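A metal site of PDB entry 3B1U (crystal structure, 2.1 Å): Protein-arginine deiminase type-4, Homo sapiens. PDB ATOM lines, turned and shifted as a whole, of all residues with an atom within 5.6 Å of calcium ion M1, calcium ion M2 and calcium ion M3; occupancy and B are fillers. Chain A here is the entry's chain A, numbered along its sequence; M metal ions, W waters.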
ATOM      1  N   ASN A 161      17.100 -32.450 -24.026  1.00  0.00           N
ATOM      2  CA  ASN A 161      17.524 -31.725 -22.824  1.00  0.00           C
ATOM      3  C   ASN A 161      17.402 -32.632 -21.596  1.00  0.00           C
ATOM      4  O   ASN A 161      16.586 -32.404 -20.696  1.00  0.00           O
ATOM      5  CB  ASN A 161      16.693 -30.449 -22.666  1.00  0.00           C
ATOM      6  CG  ASN A 161      17.296 -29.461 -21.678  1.00  0.00           C
ATOM      7  OD1 ASN A 161      18.396 -29.657 -21.154  1.00  0.00           O
ATOM      8  ND2 ASN A 161      16.569 -28.382 -21.410  1.00  0.00           N
ATOM      9  N   ASP A 163      19.830 -33.523 -19.308  1.00  0.00           N
ATOM     10  CA  ASP A 163      20.685 -33.264 -18.155  1.00  0.00           C
ATOM     11  C   ASP A 163      19.912 -32.470 -17.110  1.00  0.00           C
ATOM     12  O   ASP A 163      18.714 -32.247 -17.257  1.00  0.00           O
ATOM     13  CB  ASP A 163      21.985 -32.559 -18.586  1.00  0.00           C
ATOM     14  CG  ASP A 163      21.767 -31.095 -18.955  1.00  0.00           C
ATOM     15  OD1 ASP A 163      20.653 -30.731 -19.364  1.00  0.00           O
ATOM     16  OD2 ASP A 163      22.741 -30.316 -18.852  1.00  0.00           O
ATOM     17  N   ARG A 164      20.594 -32.062 -16.040  1.00  0.00           N
ATOM     18  CA  ARG A 164      19.956 -31.338 -14.948  1.00  0.00           C
ATOM     19  C   ARG A 164      20.801 -30.154 -14.471  1.00  0.00           C
ATOM     20  O   ARG A 164      21.587 -30.270 -13.529  1.00  0.00           O
ATOM     21  CB  ARG A 164      19.683 -32.292 -13.779  1.00  0.00           C
ATOM     22  CG  ARG A 164      18.794 -31.729 -12.695  1.00  0.00           C
ATOM     23  CD  ARG A 164      18.603 -32.754 -11.595  1.00  0.00           C
ATOM     24  NE  ARG A 164      19.794 -32.860 -10.754  1.00  0.00           N
ATOM     25  CZ  ARG A 164      20.263 -33.974 -10.208  1.00  0.00           C
ATOM     26  NH1 ARG A 164      19.672 -35.156 -10.406  1.00  0.00           N
ATOM     27  NH2 ARG A 164      21.361 -33.922  -9.464  1.00  0.00           N
ATOM     28  N   ASP A 165      20.644 -29.019 -15.147  1.00  0.00           N
ATOM     29  CA  ASP A 165      21.352 -27.783 -14.786  1.00  0.00           C
ATOM     30  C   ASP A 165      20.752 -27.138 -13.544  1.00  0.00           C
ATOM     31  O   ASP A 165      21.442 -26.431 -12.806  1.00  0.00           O
ATOM     32  CB  ASP A 165      21.325 -26.790 -15.941  1.00  0.00           C
ATOM     33  CG  ASP A 165      22.066 -27.297 -17.149  1.00  0.00           C
ATOM     34  OD1 ASP A 165      23.269 -27.618 -17.032  1.00  0.00           O
ATOM     35  OD2 ASP A 165      21.460 -27.369 -18.240  1.00  0.00           O
ATOM     36  N   ASP A 173      15.687 -31.488 -16.916  1.00  0.00           N
ATOM     37  CA  ASP A 173      15.214 -30.137 -17.234  1.00  0.00           C
ATOM     38  C   ASP A 173      13.999 -30.136 -18.168  1.00  0.00           C
ATOM     39  O   ASP A 173      13.162 -29.228 -18.083  1.00  0.00           O
ATOM     40  CB  ASP A 173      16.344 -29.304 -17.853  1.00  0.00           C
ATOM     41  CG  ASP A 173      17.507 -29.074 -16.895  1.00  0.00           C
ATOM     42  OD1 ASP A 173      17.293 -29.040 -15.665  1.00  0.00           O
ATOM     43  OD2 ASP A 173      18.653 -28.897 -17.381  1.00  0.00           O
ATOM     44  N   CYS A 174      13.904 -31.128 -19.056  1.00  0.00           N
ATOM     45  CA  CYS A 174      12.833 -31.182 -20.059  1.00  0.00           C
ATOM     46  C   CYS A 174      11.489 -31.756 -19.555  1.00  0.00           C
ATOM     47  O   CYS A 174      10.528 -31.828 -20.315  1.00  0.00           O
ATOM     48  CB  CYS A 174      13.292 -31.982 -21.276  1.00  0.00           C
ATOM     49  SG  CYS A 174      13.588 -33.736 -20.977  1.00  0.00           S
ATOM     50  N   GLU A 175      11.437 -32.163 -18.289  1.00  0.00           N
ATOM     51  CA  GLU A 175      10.217 -32.755 -17.722  1.00  0.00           C
ATOM     52  C   GLU A 175       9.135 -31.719 -17.362  1.00  0.00           C
ATOM     53  O   GLU A 175       7.968 -32.079 -17.237  1.00  0.00           O
ATOM     54  CB  GLU A 175      10.555 -33.599 -16.491  1.00  0.00           C
ATOM     55  CG  GLU A 175      11.303 -34.883 -16.827  1.00  0.00           C
ATOM     56  CD  GLU A 175      11.611 -35.729 -15.594  1.00  0.00           C
ATOM     57  OE1 GLU A 175      10.719 -35.874 -14.733  1.00  0.00           O
ATOM     58  OE2 GLU A 175      12.741 -36.258 -15.501  1.00  0.00           O
ATOM     59  N   ASP A 176       9.526 -30.450 -17.193  1.00  0.00           N
ATOM     60  CA  ASP A 176       8.565 -29.372 -16.948  1.00  0.00           C
ATOM     61  C   ASP A 176       8.462 -28.462 -18.179  1.00  0.00           C
ATOM     62  O   ASP A 176       9.125 -28.710 -19.184  1.00  0.00           O
ATOM     63  CB  ASP A 176       8.953 -28.560 -15.690  1.00  0.00           C
ATOM     64  CG  ASP A 176      10.222 -27.747 -15.867  1.00  0.00           C
ATOM     65  OD1 ASP A 176      10.628 -27.073 -14.894  1.00  0.00           O
ATOM     66  OD2 ASP A 176      10.833 -27.765 -16.962  1.00  0.00           O
ATOM     67  N   ASP A 177       7.636 -27.430 -18.097  1.00  0.00           N
ATOM     68  CA  ASP A 177       7.458 -26.486 -19.211  1.00  0.00           C
ATOM     69  C   ASP A 177       7.918 -25.070 -18.831  1.00  0.00           C
ATOM     70  O   ASP A 177       7.216 -24.084 -19.098  1.00  0.00           O
ATOM     71  CB  ASP A 177       6.023 -26.508 -19.744  1.00  0.00           C
ATOM     72  CG  ASP A 177       4.983 -26.550 -18.640  1.00  0.00           C
ATOM     73  OD1 ASP A 177       4.778 -25.519 -17.968  1.00  0.00           O
ATOM     74  OD2 ASP A 177       4.361 -27.623 -18.456  1.00  0.00           O
ATOM     75  N   GLU A 178       9.104 -24.985 -18.243  1.00  0.00           N
ATOM     76  CA  GLU A 178       9.736 -23.716 -17.880  1.00  0.00           C
ATOM     77  C   GLU A 178      11.251 -23.792 -18.072  1.00  0.00           C
ATOM     78  O   GLU A 178      11.844 -24.858 -17.929  1.00  0.00           O
ATOM     79  CB  GLU A 178       9.445 -23.356 -16.420  1.00  0.00           C
ATOM     80  CG  GLU A 178       7.976 -23.307 -16.036  1.00  0.00           C
ATOM     81  CD  GLU A 178       7.765 -22.819 -14.613  1.00  0.00           C
ATOM     82  OE1 GLU A 178       8.308 -21.762 -14.252  1.00  0.00           O
ATOM     83  OE2 GLU A 178       7.034 -23.504 -13.855  1.00  0.00           O
ATOM     84  N   VAL A 179      11.864 -22.648 -18.386  1.00  0.00           N
ATOM     85  CA  VAL A 179      13.327 -22.532 -18.383  1.00  0.00           C
ATOM     86  C   VAL A 179      13.749 -21.958 -17.026  1.00  0.00           C
ATOM     87  O   VAL A 179      13.658 -20.755 -16.800  1.00  0.00           O
ATOM     88  CB  VAL A 179      13.829 -21.619 -19.516  1.00  0.00           C
ATOM     89  CG1 VAL A 179      15.345 -21.488 -19.470  1.00  0.00           C
ATOM     90  CG2 VAL A 179      13.381 -22.150 -20.869  1.00  0.00           C
ATOM     91  N   LEU A 180      14.214 -22.834 -16.138  1.00  0.00           N
ATOM     92  CA  LEU A 180      14.515 -22.460 -14.752  1.00  0.00           C
ATOM     93  C   LEU A 180      15.867 -21.756 -14.586  1.00  0.00           C
ATOM     94  O   LEU A 180      16.011 -20.906 -13.706  1.00  0.00           O
ATOM     95  CB  LEU A 180      14.447 -23.679 -13.832  1.00  0.00           C
ATOM     96  CG  LEU A 180      13.047 -24.270 -13.615  1.00  0.00           C
ATOM     97  CD1 LEU A 180      13.139 -25.601 -12.879  1.00  0.00           C
ATOM     98  CD2 LEU A 180      12.159 -23.290 -12.855  1.00  0.00           C
ATOM     99  N   GLU A 183      21.683 -21.046 -17.767  1.00  0.00           N
ATOM    100  CA  GLU A 183      22.631 -22.026 -18.316  1.00  0.00           C
ATOM    101  C   GLU A 183      21.928 -23.105 -19.134  1.00  0.00           C
ATOM    102  O   GLU A 183      22.501 -23.657 -20.071  1.00  0.00           O
ATOM    103  CB  GLU A 183      23.456 -22.686 -17.201  1.00  0.00           C
ATOM    104  CG  GLU A 183      24.412 -21.758 -16.457  1.00  0.00           C
ATOM    105  CD  GLU A 183      23.763 -20.990 -15.312  1.00  0.00           C
ATOM    106  OE1 GLU A 183      24.433 -20.099 -14.740  1.00  0.00           O
ATOM    107  OE2 GLU A 183      22.597 -21.265 -14.977  1.00  0.00           O
ATOM    108  N   ASP A 184      20.686 -23.409 -18.759  1.00  0.00           N
ATOM    109  CA  ASP A 184      19.856 -24.399 -19.448  1.00  0.00           C
ATOM    110  C   ASP A 184      19.659 -24.064 -20.941  1.00  0.00           C
ATOM    111  O   ASP A 184      19.566 -24.963 -21.769  1.00  0.00           O
ATOM    112  CB  ASP A 184      18.495 -24.528 -18.757  1.00  0.00           C
ATOM    113  CG  ASP A 184      17.649 -25.675 -19.303  1.00  0.00           C
ATOM    114  OD1 ASP A 184      16.431 -25.485 -19.473  1.00  0.00           O
ATOM    115  OD2 ASP A 184      18.214 -26.767 -19.555  1.00  0.00           O
ATOM    116  N   ASP A 187      21.878 -25.612 -23.788  1.00  0.00           N
ATOM    117  CA  ASP A 187      21.539 -26.927 -24.334  1.00  0.00           C
ATOM    118  C   ASP A 187      20.511 -26.864 -25.456  1.00  0.00           C
ATOM    119  O   ASP A 187      20.346 -27.840 -26.190  1.00  0.00           O
ATOM    120  CB  ASP A 187      20.996 -27.827 -23.228  1.00  0.00           C
ATOM    121  CG  ASP A 187      22.004 -28.098 -22.142  1.00  0.00           C
ATOM    122  OD1 ASP A 187      23.219 -28.112 -22.417  1.00  0.00           O
ATOM    123  OD2 ASP A 187      21.574 -28.293 -20.986  1.00  0.00           O
ATOM    124  N   MET A 188      19.825 -25.739 -25.591  1.00  0.00           N
ATOM    125  CA  MET A 188      18.721 -25.606 -26.551  1.00  0.00           C
ATOM    126  C   MET A 188      19.189 -25.030 -27.874  1.00  0.00           C
ATOM    127  O   MET A 188      20.223 -24.361 -27.941  1.00  0.00           O
ATOM    128  CB  MET A 188      17.622 -24.729 -25.947  1.00  0.00           C
ATOM    129  CG  MET A 188      17.082 -25.260 -24.630  1.00  0.00           C
ATOM    130  SD  MET A 188      15.603 -24.396 -24.085  1.00  0.00           S
ATOM    131  CE  MET A 188      15.487 -24.975 -22.398  1.00  0.00           C
ATOM    132  N   PHE A 222      10.351 -22.372 -26.455  1.00  0.00           N
ATOM    133  CA  PHE A 222      10.194 -21.204 -25.589  1.00  0.00           C
ATOM    134  C   PHE A 222      10.425 -19.928 -26.388  1.00  0.00           C
ATOM    135  O   PHE A 222      11.284 -19.898 -27.274  1.00  0.00           O
ATOM    136  CB  PHE A 222      11.194 -21.243 -24.432  1.00  0.00           C
ATOM    137  CG  PHE A 222      11.039 -22.445 -23.535  1.00  0.00           C
ATOM    138  CD1 PHE A 222      11.747 -23.608 -23.797  1.00  0.00           C
ATOM    139  CD2 PHE A 222      10.190 -22.408 -22.437  1.00  0.00           C
ATOM    140  CE1 PHE A 222      11.615 -24.722 -22.978  1.00  0.00           C
ATOM    141  CE2 PHE A 222      10.053 -23.512 -21.618  1.00  0.00           C
ATOM    142  CZ  PHE A 222      10.758 -24.666 -21.881  1.00  0.00           C
ATOM    143  N   GLU A 260      13.969 -27.322 -27.340  1.00  0.00           N
ATOM    144  CA  GLU A 260      14.530 -28.519 -26.706  1.00  0.00           C
ATOM    145  C   GLU A 260      13.786 -29.757 -27.170  1.00  0.00           C
ATOM    146  O   GLU A 260      12.570 -29.702 -27.394  1.00  0.00           O
ATOM    147  CB  GLU A 260      14.458 -28.408 -25.175  1.00  0.00           C
ATOM    148  CG  GLU A 260      13.046 -28.233 -24.619  1.00  0.00           C
ATOM    149  CD  GLU A 260      12.984 -28.207 -23.100  1.00  0.00           C
ATOM    150  OE1 GLU A 260      14.051 -28.058 -22.459  1.00  0.00           O
ATOM    151  OE2 GLU A 260      11.874 -28.341 -22.551  1.00  0.00           O
ATOM    152  N   LYS A 370      26.550 -27.324 -28.642  1.00  0.00           N
ATOM    153  CA  LYS A 370      26.708 -27.965 -27.335  1.00  0.00           C
ATOM    154  C   LYS A 370      26.948 -29.475 -27.441  1.00  0.00           C
ATOM    155  O   LYS A 370      26.303 -30.177 -28.219  1.00  0.00           O
ATOM    156  CB  LYS A 370      25.467 -27.691 -26.477  1.00  0.00           C
ATOM    157  CG  LYS A 370      25.447 -28.368 -25.108  1.00  0.00           C
ATOM    158  CD  LYS A 370      26.517 -27.819 -24.161  1.00  0.00           C
ATOM    159  CE  LYS A 370      26.137 -26.458 -23.609  1.00  0.00           C
ATOM    160  NZ  LYS A 370      27.100 -25.980 -22.579  1.00  0.00           N
ATOM    161  N   LEU A 372      27.525 -32.748 -24.582  1.00  0.00           N
ATOM    162  CA  LEU A 372      27.557 -33.183 -23.184  1.00  0.00           C
ATOM    163  C   LEU A 372      27.512 -34.703 -23.050  1.00  0.00           C
ATOM    164  O   LEU A 372      26.918 -35.379 -23.885  1.00  0.00           O
ATOM    165  CB  LEU A 372      26.398 -32.564 -22.391  1.00  0.00           C
ATOM    166  CG  LEU A 372      24.971 -32.787 -22.898  1.00  0.00           C
ATOM    167  CD1 LEU A 372      23.970 -32.830 -21.741  1.00  0.00           C
ATOM    168  CD2 LEU A 372      24.579 -31.716 -23.903  1.00  0.00           C
ATOM    169  N   PRO A 395      24.472 -31.332 -13.791  1.00  0.00           N
ATOM    170  CA  PRO A 395      24.835 -30.228 -14.693  1.00  0.00           C
ATOM    171  C   PRO A 395      25.743 -30.669 -15.838  1.00  0.00           C
ATOM    172  O   PRO A 395      26.860 -31.135 -15.602  1.00  0.00           O
ATOM    173  CB  PRO A 395      25.565 -29.245 -13.751  1.00  0.00           C
ATOM    174  CG  PRO A 395      25.002 -29.523 -12.408  1.00  0.00           C
ATOM    175  CD  PRO A 395      24.730 -30.996 -12.382  1.00  0.00           C
ATOM    176  N   ASP A 396      25.245 -30.524 -17.066  1.00  0.00           N
ATOM    177  CA  ASP A 396      25.949 -30.981 -18.277  1.00  0.00           C
ATOM    178  C   ASP A 396      26.282 -32.482 -18.249  1.00  0.00           C
ATOM    179  O   ASP A 396      27.297 -32.912 -18.803  1.00  0.00           O
ATOM    180  CB  ASP A 396      27.219 -30.143 -18.536  1.00  0.00           C
ATOM    181  CG  ASP A 396      26.903 -28.697 -18.894  1.00  0.00           C
ATOM    182  OD1 ASP A 396      25.810 -28.436 -19.449  1.00  0.00           O
ATOM    183  OD2 ASP A 396      27.733 -27.811 -18.621  1.00  0.00           O
HETATM  184 CA    CA M   1      19.766 -28.508 -19.544  1.00  0.00          CA
HETATM  185 CA    CA M   2      23.583 -28.155 -19.580  1.00  0.00          CA
HETATM  186 CA    CA M   3      12.791 -26.937 -18.116  1.00  0.00          CA
HETATM  187  O   HOH W   1      23.934 -25.914 -19.440  1.00  0.00           O
HETATM  188  O   HOH W   2      14.177 -26.937 -19.959  1.00  0.00           O
HETATM  189  O   HOH W   3      11.367 -27.536 -19.999  1.00  0.00           O
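Calcium ion M2 is bound by OD1 of Asp 396 (2.2 Å).
Calcium ion M2 is bound by water W1 (2.3 Å).
The side-chain carboxylate (OD2) of Asp 163 binds calcium ion M2 (2.4 Å).
OD2 of Asp 187 binds calcium ion M2, at 2.5 Å.
OD1 of Asp 165 binds calcium ion M2.
Calcium ion M2 is bound by OD2 of Asp 165 (2.6 Å).
Calcium ion M2 is bound by the side-chain carboxylate (OD1) of Asp 187 (2.9 Å).
Calcium ion M2 has seven donor atoms within binding distance.
Calcium ion M1 is bound by the side-chain carboxylate of Asp 187 (2.3 Å), the side-chain carboxylate of Asp 184 (2.3 Å), the side-chain carboxylate of Asp 163 (2.4 Å), the side-chain amide oxygen of Asn 161 (2.4 Å), the side-chain carboxylate of Asp 165 (2.4 Å) and the side-chain carboxylate of Asp 173 (2.5 Å).
O of Asn 161 is in hydrogen-bond range of SG of Cys 174.
The side-chain amide nitrogen (ND2) of Asn 161 is in hydrogen-bond range of the side-chain carboxylate (OE1) of Glu 260 (2.7 Å).
Calcium ion M3 is bound by O of Glu 178, water W2, O of Asp 173, OD2 of Asp 176 and water W3.
Calcium ion M3 has five donor atoms within binding distance.
Water W2 lies within hydrogen-bond range of OD1 of Asp 184, OE1 of Glu 260 and ND2 of Asn 161.
Water W3 lies within hydrogen-bond range of the backbone carbonyl oxygen of Asp 176 (2.7 Å) and the side-chain carboxylate of Glu 260 (2.7 Å).
The nearest printed residue that does not touch calcium ion M3 is Asp 184 (4.1 Å).
Four residues have an atom within 4 Å of calcium ion M2: Asp 163, Asp 165, Asp 187 and Asp 396.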
